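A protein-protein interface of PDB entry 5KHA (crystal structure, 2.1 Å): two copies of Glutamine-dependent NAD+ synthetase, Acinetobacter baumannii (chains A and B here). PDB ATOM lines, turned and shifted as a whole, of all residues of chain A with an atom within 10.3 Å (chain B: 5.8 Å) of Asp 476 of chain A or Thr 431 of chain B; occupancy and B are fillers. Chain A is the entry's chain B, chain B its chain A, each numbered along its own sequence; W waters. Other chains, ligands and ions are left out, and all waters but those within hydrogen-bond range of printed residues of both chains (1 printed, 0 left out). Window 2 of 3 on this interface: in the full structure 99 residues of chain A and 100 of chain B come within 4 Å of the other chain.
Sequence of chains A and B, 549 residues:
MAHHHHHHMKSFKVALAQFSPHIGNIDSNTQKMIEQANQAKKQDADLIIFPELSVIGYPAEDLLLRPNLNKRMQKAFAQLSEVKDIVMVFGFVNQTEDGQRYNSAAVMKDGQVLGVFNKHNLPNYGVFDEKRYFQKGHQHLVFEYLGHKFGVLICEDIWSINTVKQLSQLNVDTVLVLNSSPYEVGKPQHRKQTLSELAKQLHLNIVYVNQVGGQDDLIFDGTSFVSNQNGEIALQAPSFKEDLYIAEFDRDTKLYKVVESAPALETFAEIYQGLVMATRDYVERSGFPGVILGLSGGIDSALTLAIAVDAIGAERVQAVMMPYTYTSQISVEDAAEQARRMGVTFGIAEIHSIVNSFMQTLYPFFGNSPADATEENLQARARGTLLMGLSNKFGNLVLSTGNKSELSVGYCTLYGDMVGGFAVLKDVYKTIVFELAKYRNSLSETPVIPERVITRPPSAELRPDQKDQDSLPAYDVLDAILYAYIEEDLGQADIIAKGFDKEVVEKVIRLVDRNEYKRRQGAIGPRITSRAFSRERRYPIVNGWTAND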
ATOM      1  N   LEU A 472     -20.482 -13.994 -20.801  1.00  0.00           N
ATOM      2  CA  LEU A 472     -21.426 -13.320 -19.931  1.00  0.00           C
ATOM      3  C   LEU A 472     -22.821 -13.295 -20.548  1.00  0.00           C
ATOM      4  O   LEU A 472     -22.980 -13.417 -21.763  1.00  0.00           O
ATOM      5  CB  LEU A 472     -20.952 -11.899 -19.664  1.00  0.00           C
ATOM      6  CG  LEU A 472     -19.667 -11.841 -18.839  1.00  0.00           C
ATOM      7  CD1 LEU A 472     -19.155 -10.410 -18.766  1.00  0.00           C
ATOM      8  CD2 LEU A 472     -19.889 -12.419 -17.453  1.00  0.00           C
ATOM      9  N   PRO A 473     -23.853 -13.106 -19.736  1.00  0.00           N
ATOM     10  CA  PRO A 473     -25.208 -12.995 -20.289  1.00  0.00           C
ATOM     11  C   PRO A 473     -25.358 -11.708 -21.089  1.00  0.00           C
ATOM     12  O   PRO A 473     -24.491 -10.837 -21.088  1.00  0.00           O
ATOM     13  CB  PRO A 473     -26.110 -13.015 -19.048  1.00  0.00           C
ATOM     14  CG  PRO A 473     -25.213 -12.641 -17.907  1.00  0.00           C
ATOM     15  CD  PRO A 473     -23.847 -13.125 -18.261  1.00  0.00           C
ATOM     16  N   ALA A 474     -26.467 -11.610 -21.819  1.00  0.00           N
ATOM     17  CA  ALA A 474     -26.756 -10.372 -22.529  1.00  0.00           C
ATOM     18  C   ALA A 474     -26.929  -9.203 -21.547  1.00  0.00           C
ATOM     19  O   ALA A 474     -27.201  -9.375 -20.349  1.00  0.00           O
ATOM     20  CB  ALA A 474     -27.989 -10.543 -23.418  1.00  0.00           C
ATOM     21  N   TYR A 475     -26.771  -7.992 -22.077  1.00  0.00           N
ATOM     22  CA  TYR A 475     -26.698  -6.814 -21.214  1.00  0.00           C
ATOM     23  C   TYR A 475     -27.930  -6.643 -20.331  1.00  0.00           C
ATOM     24  O   TYR A 475     -27.821  -6.101 -19.224  1.00  0.00           O
ATOM     25  CB  TYR A 475     -26.463  -5.560 -22.058  1.00  0.00           C
ATOM     26  CG  TYR A 475     -25.024  -5.432 -22.500  1.00  0.00           C
ATOM     27  CD1 TYR A 475     -24.032  -5.091 -21.589  1.00  0.00           C
ATOM     28  CD2 TYR A 475     -24.651  -5.668 -23.815  1.00  0.00           C
ATOM     29  CE1 TYR A 475     -22.715  -4.979 -21.975  1.00  0.00           C
ATOM     30  CE2 TYR A 475     -23.335  -5.558 -24.213  1.00  0.00           C
ATOM     31  CZ  TYR A 475     -22.369  -5.212 -23.285  1.00  0.00           C
ATOM     32  OH  TYR A 475     -21.048  -5.103 -23.661  1.00  0.00           O
ATOM     33  N   ASP A 476     -29.109  -7.080 -20.778  1.00  0.00           N
ATOM     34  CA  ASP A 476     -30.280  -6.843 -19.934  1.00  0.00           C
ATOM     35  C   ASP A 476     -30.218  -7.683 -18.656  1.00  0.00           C
ATOM     36  O   ASP A 476     -30.513  -7.185 -17.562  1.00  0.00           O
ATOM     37  CB  ASP A 476     -31.575  -7.084 -20.721  1.00  0.00           C
ATOM     38  CG  ASP A 476     -31.852  -8.550 -20.980  1.00  0.00           C
ATOM     39  OD1 ASP A 476     -31.070  -9.185 -21.719  1.00  0.00           O
ATOM     40  OD2 ASP A 476     -32.866  -9.066 -20.451  1.00  0.00           O
ATOM     41  N   VAL A 477     -29.799  -8.943 -18.764  1.00  0.00           N
ATOM     42  CA  VAL A 477     -29.570  -9.762 -17.576  1.00  0.00           C
ATOM     43  C   VAL A 477     -28.331  -9.291 -16.821  1.00  0.00           C
ATOM     44  O   VAL A 477     -28.331  -9.204 -15.587  1.00  0.00           O
ATOM     45  CB  VAL A 477     -29.456 -11.241 -17.973  1.00  0.00           C
ATOM     46  CG1 VAL A 477     -28.936 -12.067 -16.800  1.00  0.00           C
ATOM     47  CG2 VAL A 477     -30.806 -11.741 -18.486  1.00  0.00           C
ATOM     48  N   LEU A 478     -27.235  -9.047 -17.543  1.00  0.00           N
ATOM     49  CA  LEU A 478     -26.004  -8.628 -16.883  1.00  0.00           C
ATOM     50  C   LEU A 478     -26.215  -7.359 -16.055  1.00  0.00           C
ATOM     51  O   LEU A 478     -25.721  -7.257 -14.924  1.00  0.00           O
ATOM     52  CB  LEU A 478     -24.892  -8.431 -17.921  1.00  0.00           C
ATOM     53  CG  LEU A 478     -23.615  -7.772 -17.382  1.00  0.00           C
ATOM     54  CD1 LEU A 478     -22.919  -8.646 -16.323  1.00  0.00           C
ATOM     55  CD2 LEU A 478     -22.644  -7.405 -18.529  1.00  0.00           C
ATOM     56  N   ASP A 479     -26.943  -6.379 -16.605  1.00  0.00           N
ATOM     57  CA  ASP A 479     -27.108  -5.108 -15.908  1.00  0.00           C
ATOM     58  C   ASP A 479     -27.996  -5.250 -14.685  1.00  0.00           C
ATOM     59  O   ASP A 479     -27.798  -4.525 -13.702  1.00  0.00           O
ATOM     60  CB  ASP A 479     -27.665  -4.043 -16.851  1.00  0.00           C
ATOM     61  CG  ASP A 479     -26.650  -3.612 -17.892  1.00  0.00           C
ATOM     62  OD1 ASP A 479     -25.480  -4.002 -17.761  1.00  0.00           O
ATOM     63  OD2 ASP A 479     -27.009  -2.894 -18.842  1.00  0.00           O
ATOM     64  N   ALA A 480     -28.969  -6.176 -14.722  1.00  0.00           N
ATOM     65  CA  ALA A 480     -29.771  -6.442 -13.531  1.00  0.00           C
ATOM     66  C   ALA A 480     -28.923  -7.041 -12.414  1.00  0.00           C
ATOM     67  O   ALA A 480     -29.075  -6.666 -11.242  1.00  0.00           O
ATOM     68  CB  ALA A 480     -30.962  -7.351 -13.867  1.00  0.00           C
ATOM     69  N   ILE A 481     -28.026  -7.973 -12.748  1.00  0.00           N
ATOM     70  CA  ILE A 481     -27.150  -8.543 -11.723  1.00  0.00           C
ATOM     71  C   ILE A 481     -26.195  -7.477 -11.165  1.00  0.00           C
ATOM     72  O   ILE A 481     -25.956  -7.406  -9.952  1.00  0.00           O
ATOM     73  CB  ILE A 481     -26.391  -9.758 -12.294  1.00  0.00           C
ATOM     74  CG1 ILE A 481     -27.379 -10.905 -12.587  1.00  0.00           C
ATOM     75  CG2 ILE A 481     -25.302 -10.222 -11.338  1.00  0.00           C
ATOM     76  CD1 ILE A 481     -26.749 -12.070 -13.335  1.00  0.00           C
ATOM     77  N   LEU A 482     -25.629  -6.643 -12.037  1.00  0.00           N
ATOM     78  CA  LEU A 482     -24.738  -5.579 -11.577  1.00  0.00           C
ATOM     79  C   LEU A 482     -25.471  -4.578 -10.690  1.00  0.00           C
ATOM     80  O   LEU A 482     -24.957  -4.172  -9.640  1.00  0.00           O
ATOM     81  CB  LEU A 482     -24.116  -4.862 -12.773  1.00  0.00           C
ATOM     82  CG  LEU A 482     -23.185  -5.661 -13.693  1.00  0.00           C
ATOM     83  CD1 LEU A 482     -22.881  -4.848 -14.928  1.00  0.00           C
ATOM     84  CD2 LEU A 482     -21.898  -6.049 -12.952  1.00  0.00           C
ATOM     85  N   TYR A 483     -26.672  -4.161 -11.096  1.00  0.00           N
ATOM     86  CA  TYR A 483     -27.438  -3.240 -10.260  1.00  0.00           C
ATOM     87  C   TYR A 483     -27.656  -3.830  -8.872  1.00  0.00           C
ATOM     88  O   TYR A 483     -27.493  -3.144  -7.869  1.00  0.00           O
ATOM     89  CB  TYR A 483     -28.783  -2.919 -10.920  1.00  0.00           C
ATOM     90  CG  TYR A 483     -29.597  -1.912 -10.150  1.00  0.00           C
ATOM     91  CD1 TYR A 483     -29.440  -0.549 -10.373  1.00  0.00           C
ATOM     92  CD2 TYR A 483     -30.518  -2.323  -9.178  1.00  0.00           C
ATOM     93  CE1 TYR A 483     -30.186   0.376  -9.659  1.00  0.00           C
ATOM     94  CE2 TYR A 483     -31.247  -1.405  -8.460  1.00  0.00           C
ATOM     95  CZ  TYR A 483     -31.076  -0.058  -8.704  1.00  0.00           C
ATOM     96  OH  TYR A 483     -31.807   0.871  -7.990  1.00  0.00           O
ATOM     97  N   ALA A 484     -27.961  -5.123  -8.808  1.00  0.00           N
ATOM     98  CA  ALA A 484     -28.182  -5.789  -7.531  1.00  0.00           C
ATOM     99  C   ALA A 484     -26.915  -5.809  -6.670  1.00  0.00           C
ATOM    100  O   ALA A 484     -26.980  -5.628  -5.449  1.00  0.00           O
ATOM    101  CB  ALA A 484     -28.703  -7.206  -7.796  1.00  0.00           C
ATOM    102  N   PHE A 500     -31.820 -15.427 -10.656  1.00  0.00           N
ATOM    103  CA  PHE A 500     -30.683 -15.559 -11.558  1.00  0.00           C
ATOM    104  C   PHE A 500     -29.911 -16.847 -11.274  1.00  0.00           C
ATOM    105  O   PHE A 500     -29.899 -17.353 -10.151  1.00  0.00           O
ATOM    106  CB  PHE A 500     -29.774 -14.339 -11.428  1.00  0.00           C
ATOM    107  CG  PHE A 500     -30.426 -13.075 -11.852  1.00  0.00           C
ATOM    108  CD1 PHE A 500     -30.678 -12.834 -13.196  1.00  0.00           C
ATOM    109  CD2 PHE A 500     -30.815 -12.126 -10.914  1.00  0.00           C
ATOM    110  CE1 PHE A 500     -31.302 -11.670 -13.603  1.00  0.00           C
ATOM    111  CE2 PHE A 500     -31.441 -10.947 -11.315  1.00  0.00           C
ATOM    112  CZ  PHE A 500     -31.685 -10.716 -12.655  1.00  0.00           C
ATOM    113  N   VAL A 504     -23.729 -18.037 -12.945  1.00  0.00           N
ATOM    114  CA  VAL A 504     -23.635 -16.751 -13.628  1.00  0.00           C
ATOM    115  C   VAL A 504     -23.417 -15.623 -12.625  1.00  0.00           C
ATOM    116  O   VAL A 504     -22.592 -14.736 -12.854  1.00  0.00           O
ATOM    117  CB  VAL A 504     -24.871 -16.506 -14.502  1.00  0.00           C
ATOM    118  CG1 VAL A 504     -24.859 -15.085 -15.013  1.00  0.00           C
ATOM    119  CG2 VAL A 504     -24.873 -17.502 -15.674  1.00  0.00           C
ATOM    120  N   VAL A 508     -20.131 -13.154 -12.422  1.00  0.00           N
ATOM    121  CA  VAL A 508     -20.222 -11.704 -12.544  1.00  0.00           C
ATOM    122  C   VAL A 508     -19.586 -11.021 -11.338  1.00  0.00           C
ATOM    123  O   VAL A 508     -18.808 -10.076 -11.487  1.00  0.00           O
ATOM    124  CB  VAL A 508     -21.678 -11.261 -12.744  1.00  0.00           C
ATOM    125  CG1 VAL A 508     -21.762  -9.733 -12.748  1.00  0.00           C
ATOM    126  CG2 VAL A 508     -22.192 -11.801 -14.056  1.00  0.00           C
ATOM    127  N   ILE A 528     -24.536   9.375 -12.053  1.00  0.00           N
ATOM    128  CA  ILE A 528     -25.976   9.525 -12.227  1.00  0.00           C
ATOM    129  C   ILE A 528     -26.757   8.517 -11.402  1.00  0.00           C
ATOM    130  O   ILE A 528     -27.993   8.538 -11.400  1.00  0.00           O
ATOM    131  CB  ILE A 528     -26.383   9.390 -13.699  1.00  0.00           C
ATOM    132  CG1 ILE A 528     -26.034   7.978 -14.204  1.00  0.00           C
ATOM    133  CG2 ILE A 528     -25.770  10.507 -14.536  1.00  0.00           C
ATOM    134  CD1 ILE A 528     -27.065   7.403 -15.175  1.00  0.00           C
ATOM    135  N   SER B 405     -21.500  -0.946 -17.622  1.00  0.00           N
ATOM    136  CA  SER B 405     -21.501  -2.403 -17.722  1.00  0.00           C
ATOM    137  C   SER B 405     -20.114  -2.914 -18.081  1.00  0.00           C
ATOM    138  O   SER B 405     -19.630  -3.894 -17.507  1.00  0.00           O
ATOM    139  CB  SER B 405     -22.530  -2.863 -18.754  1.00  0.00           C
ATOM    140  OG  SER B 405     -23.759  -2.152 -18.633  1.00  0.00           O
ATOM    141  N   TYR B 429     -25.163   2.329 -17.305  1.00  0.00           N
ATOM    142  CA  TYR B 429     -25.252   0.945 -17.772  1.00  0.00           C
ATOM    143  C   TYR B 429     -25.630   0.896 -19.253  1.00  0.00           C
ATOM    144  O   TYR B 429     -26.337   1.770 -19.768  1.00  0.00           O
ATOM    145  CB  TYR B 429     -26.284   0.141 -16.966  1.00  0.00           C
ATOM    146  CG  TYR B 429     -25.831  -0.232 -15.570  1.00  0.00           C
ATOM    147  CD1 TYR B 429     -24.667  -0.974 -15.376  1.00  0.00           C
ATOM    148  CD2 TYR B 429     -26.554   0.172 -14.444  1.00  0.00           C
ATOM    149  CE1 TYR B 429     -24.234  -1.307 -14.104  1.00  0.00           C
ATOM    150  CE2 TYR B 429     -26.130  -0.167 -13.154  1.00  0.00           C
ATOM    151  CZ  TYR B 429     -24.964  -0.899 -12.995  1.00  0.00           C
ATOM    152  OH  TYR B 429     -24.521  -1.236 -11.737  1.00  0.00           O
ATOM    153  N   LYS B 430     -25.145  -0.148 -19.932  1.00  0.00           N
ATOM    154  CA  LYS B 430     -25.433  -0.332 -21.353  1.00  0.00           C
ATOM    155  C   LYS B 430     -26.936  -0.294 -21.629  1.00  0.00           C
ATOM    156  O   LYS B 430     -27.386   0.310 -22.611  1.00  0.00           O
ATOM    157  CB  LYS B 430     -24.816  -1.652 -21.827  1.00  0.00           C
ATOM    158  CG  LYS B 430     -25.017  -1.958 -23.319  1.00  0.00           C
ATOM    159  CD  LYS B 430     -24.259  -0.962 -24.193  1.00  0.00           C
ATOM    160  CE  LYS B 430     -23.941  -1.579 -25.566  1.00  0.00           C
ATOM    161  NZ  LYS B 430     -22.699  -0.993 -26.148  1.00  0.00           N
ATOM    162  N   THR B 431     -27.725  -0.930 -20.764  1.00  0.00           N
ATOM    163  CA  THR B 431     -29.183  -0.830 -20.833  1.00  0.00           C
ATOM    164  C   THR B 431     -29.662   0.620 -20.892  1.00  0.00           C
ATOM    165  O   THR B 431     -30.591   0.948 -21.641  1.00  0.00           O
ATOM    166  CB  THR B 431     -29.798  -1.559 -19.634  1.00  0.00           C
ATOM    167  OG1 THR B 431     -29.546  -2.962 -19.768  1.00  0.00           O
ATOM    168  CG2 THR B 431     -31.312  -1.326 -19.560  1.00  0.00           C
ATOM    169  N   ILE B 432     -29.049   1.504 -20.104  1.00  0.00           N
ATOM    170  CA  ILE B 432     -29.461   2.905 -20.108  1.00  0.00           C
ATOM    171  C   ILE B 432     -28.969   3.602 -21.366  1.00  0.00           C
ATOM    172  O   ILE B 432     -29.622   4.526 -21.872  1.00  0.00           O
ATOM    173  CB  ILE B 432     -28.946   3.621 -18.843  1.00  0.00           C
ATOM    174  CG1 ILE B 432     -29.382   2.856 -17.590  1.00  0.00           C
ATOM    175  CG2 ILE B 432     -29.417   5.082 -18.811  1.00  0.00           C
ATOM    176  CD1 ILE B 432     -30.856   2.862 -17.363  1.00  0.00           C
ATOM    177  N   VAL B 433     -27.810   3.188 -21.876  1.00  0.00           N
ATOM    178  CA  VAL B 433     -27.275   3.773 -23.105  1.00  0.00           C
ATOM    179  C   VAL B 433     -28.299   3.679 -24.232  1.00  0.00           C
ATOM    180  O   VAL B 433     -28.577   4.668 -24.919  1.00  0.00           O
ATOM    181  CB  VAL B 433     -25.952   3.088 -23.486  1.00  0.00           C
ATOM    182  CG1 VAL B 433     -25.539   3.446 -24.937  1.00  0.00           C
ATOM    183  CG2 VAL B 433     -24.859   3.461 -22.481  1.00  0.00           C
ATOM    184  N   PHE B 434     -28.909   2.495 -24.410  1.00  0.00           N
ATOM    185  CA  PHE B 434     -29.906   2.343 -25.468  1.00  0.00           C
ATOM    186  C   PHE B 434     -31.057   3.323 -25.280  1.00  0.00           C
ATOM    187  O   PHE B 434     -31.497   3.971 -26.240  1.00  0.00           O
ATOM    188  CB  PHE B 434     -30.433   0.904 -25.507  1.00  0.00           C
ATOM    189  CG  PHE B 434     -29.490  -0.085 -26.138  1.00  0.00           C
ATOM    190  CD1 PHE B 434     -29.327  -0.135 -27.516  1.00  0.00           C
ATOM    191  CD2 PHE B 434     -28.794  -0.993 -25.356  1.00  0.00           C
ATOM    192  CE1 PHE B 434     -28.462  -1.061 -28.099  1.00  0.00           C
ATOM    193  CE2 PHE B 434     -27.929  -1.917 -25.928  1.00  0.00           C
ATOM    194  CZ  PHE B 434     -27.764  -1.953 -27.303  1.00  0.00           C
ATOM    195  N   GLU B 435     -31.540   3.470 -24.043  1.00  0.00           N
ATOM    196  CA  GLU B 435     -32.675   4.351 -23.793  1.00  0.00           C
ATOM    197  C   GLU B 435     -32.308   5.802 -24.057  1.00  0.00           C
ATOM    198  O   GLU B 435     -33.135   6.572 -24.554  1.00  0.00           O
ATOM    199  CB  GLU B 435     -33.181   4.158 -22.357  1.00  0.00           C
ATOM    200  CG  GLU B 435     -33.841   2.801 -22.122  1.00  0.00           C
ATOM    201  CD  GLU B 435     -34.828   2.451 -23.224  1.00  0.00           C
ATOM    202  OE1 GLU B 435     -35.894   3.092 -23.254  1.00  0.00           O
ATOM    203  OE2 GLU B 435     -34.532   1.572 -24.072  1.00  0.00           O
ATOM    204  N   LEU B 436     -31.064   6.187 -23.753  1.00  0.00           N
ATOM    205  CA  LEU B 436     -30.630   7.565 -23.991  1.00  0.00           C
ATOM    206  C   LEU B 436     -30.521   7.863 -25.483  1.00  0.00           C
ATOM    207  O   LEU B 436     -30.846   8.970 -25.928  1.00  0.00           O
ATOM    208  CB  LEU B 436     -29.294   7.818 -23.292  1.00  0.00           C
ATOM    209  CG  LEU B 436     -29.312   7.727 -21.759  1.00  0.00           C
ATOM    210  CD1 LEU B 436     -27.904   7.853 -21.170  1.00  0.00           C
ATOM    211  CD2 LEU B 436     -30.268   8.767 -21.143  1.00  0.00           C
HETATM  212  O   HOH W   1     -21.135  -2.297 -24.074  1.00  0.00           O
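OD1 of Asp 479 of chain A sits at hydrogen-bond distance from OG of Ser 405 of chain B (2.7 Å).
The backbone NH (N) of Lys 430 of chain B sits at hydrogen-bond distance from the side-chain carboxylate (OD2) of Asp 479 of chain A (3.5 Å).
OG1 of Thr 431 of chain B lies within hydrogen-bond range of OD2 of Asp 479 of chain A.
The side-chain hydroxyl (OG) of Ser 405 of chain B sits at hydrogen-bond distance from the backbone NH (N) of Lys 430 of chain B (2.8 Å).
CE1 of Tyr 475 of chain A touches CB of Ser 405 of chain B, at 3.9 Å.
Tyr 475 of chain A touches Lys 430 of chain B.
Tyr 475 of chain A touches Thr 431 of chain B (O to OG1, 3.6 Å).
Thr 431 of chain B touches Asp 476 of chain A (OG1 to CA, 3.95 Å).
Tyr 429 of chain B touches Asp 479 of chain A.
CA of Ser 405 of chain B touches CD1 of Leu 482 of chain A (3.96 Å).
Tyr 429 of chain B touches Leu 482 of chain A.
Tyr 483 of chain A touches Tyr 429 of chain B.
Of the printed residues of chain A, Thr 431 of chain B touches Tyr 475, Asp 476 and Asp 479.
No residue of chain A comes within 4 Å of Ile 432 of chain B.
Of the printed residues of chain B, Leu 482 of chain A touches Ser 405 and Tyr 429.
Of the printed residues of chain A, Tyr 429 of chain B touches Asp 479 (3.6 Å), Leu 482 (3.6 Å) and Tyr 483 (3.7 Å).
Of the printed residues of chain A, Ser 405 of chain B touches Tyr 475, Asp 479 and Leu 482.
Ile 528 of chain A touches none of the printed residues of chain B.
The nearest printed residue of chain A that does not touch Thr 431 of chain B is Ala 480 of chain A (6.0 Å).
Of the 9 printed residues of chain B, 4 touch a printed residue of chain A.
Among the printed residues, 11 pairs touch across the chains.
No position is printed for both chains.
Water W1 bridges the side-chain hydroxyl (OH) of Tyr 475 of chain A (2.8 Å) and the side-chain amino group (NZ) of Lys 430 of chain B (2.9 Å).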
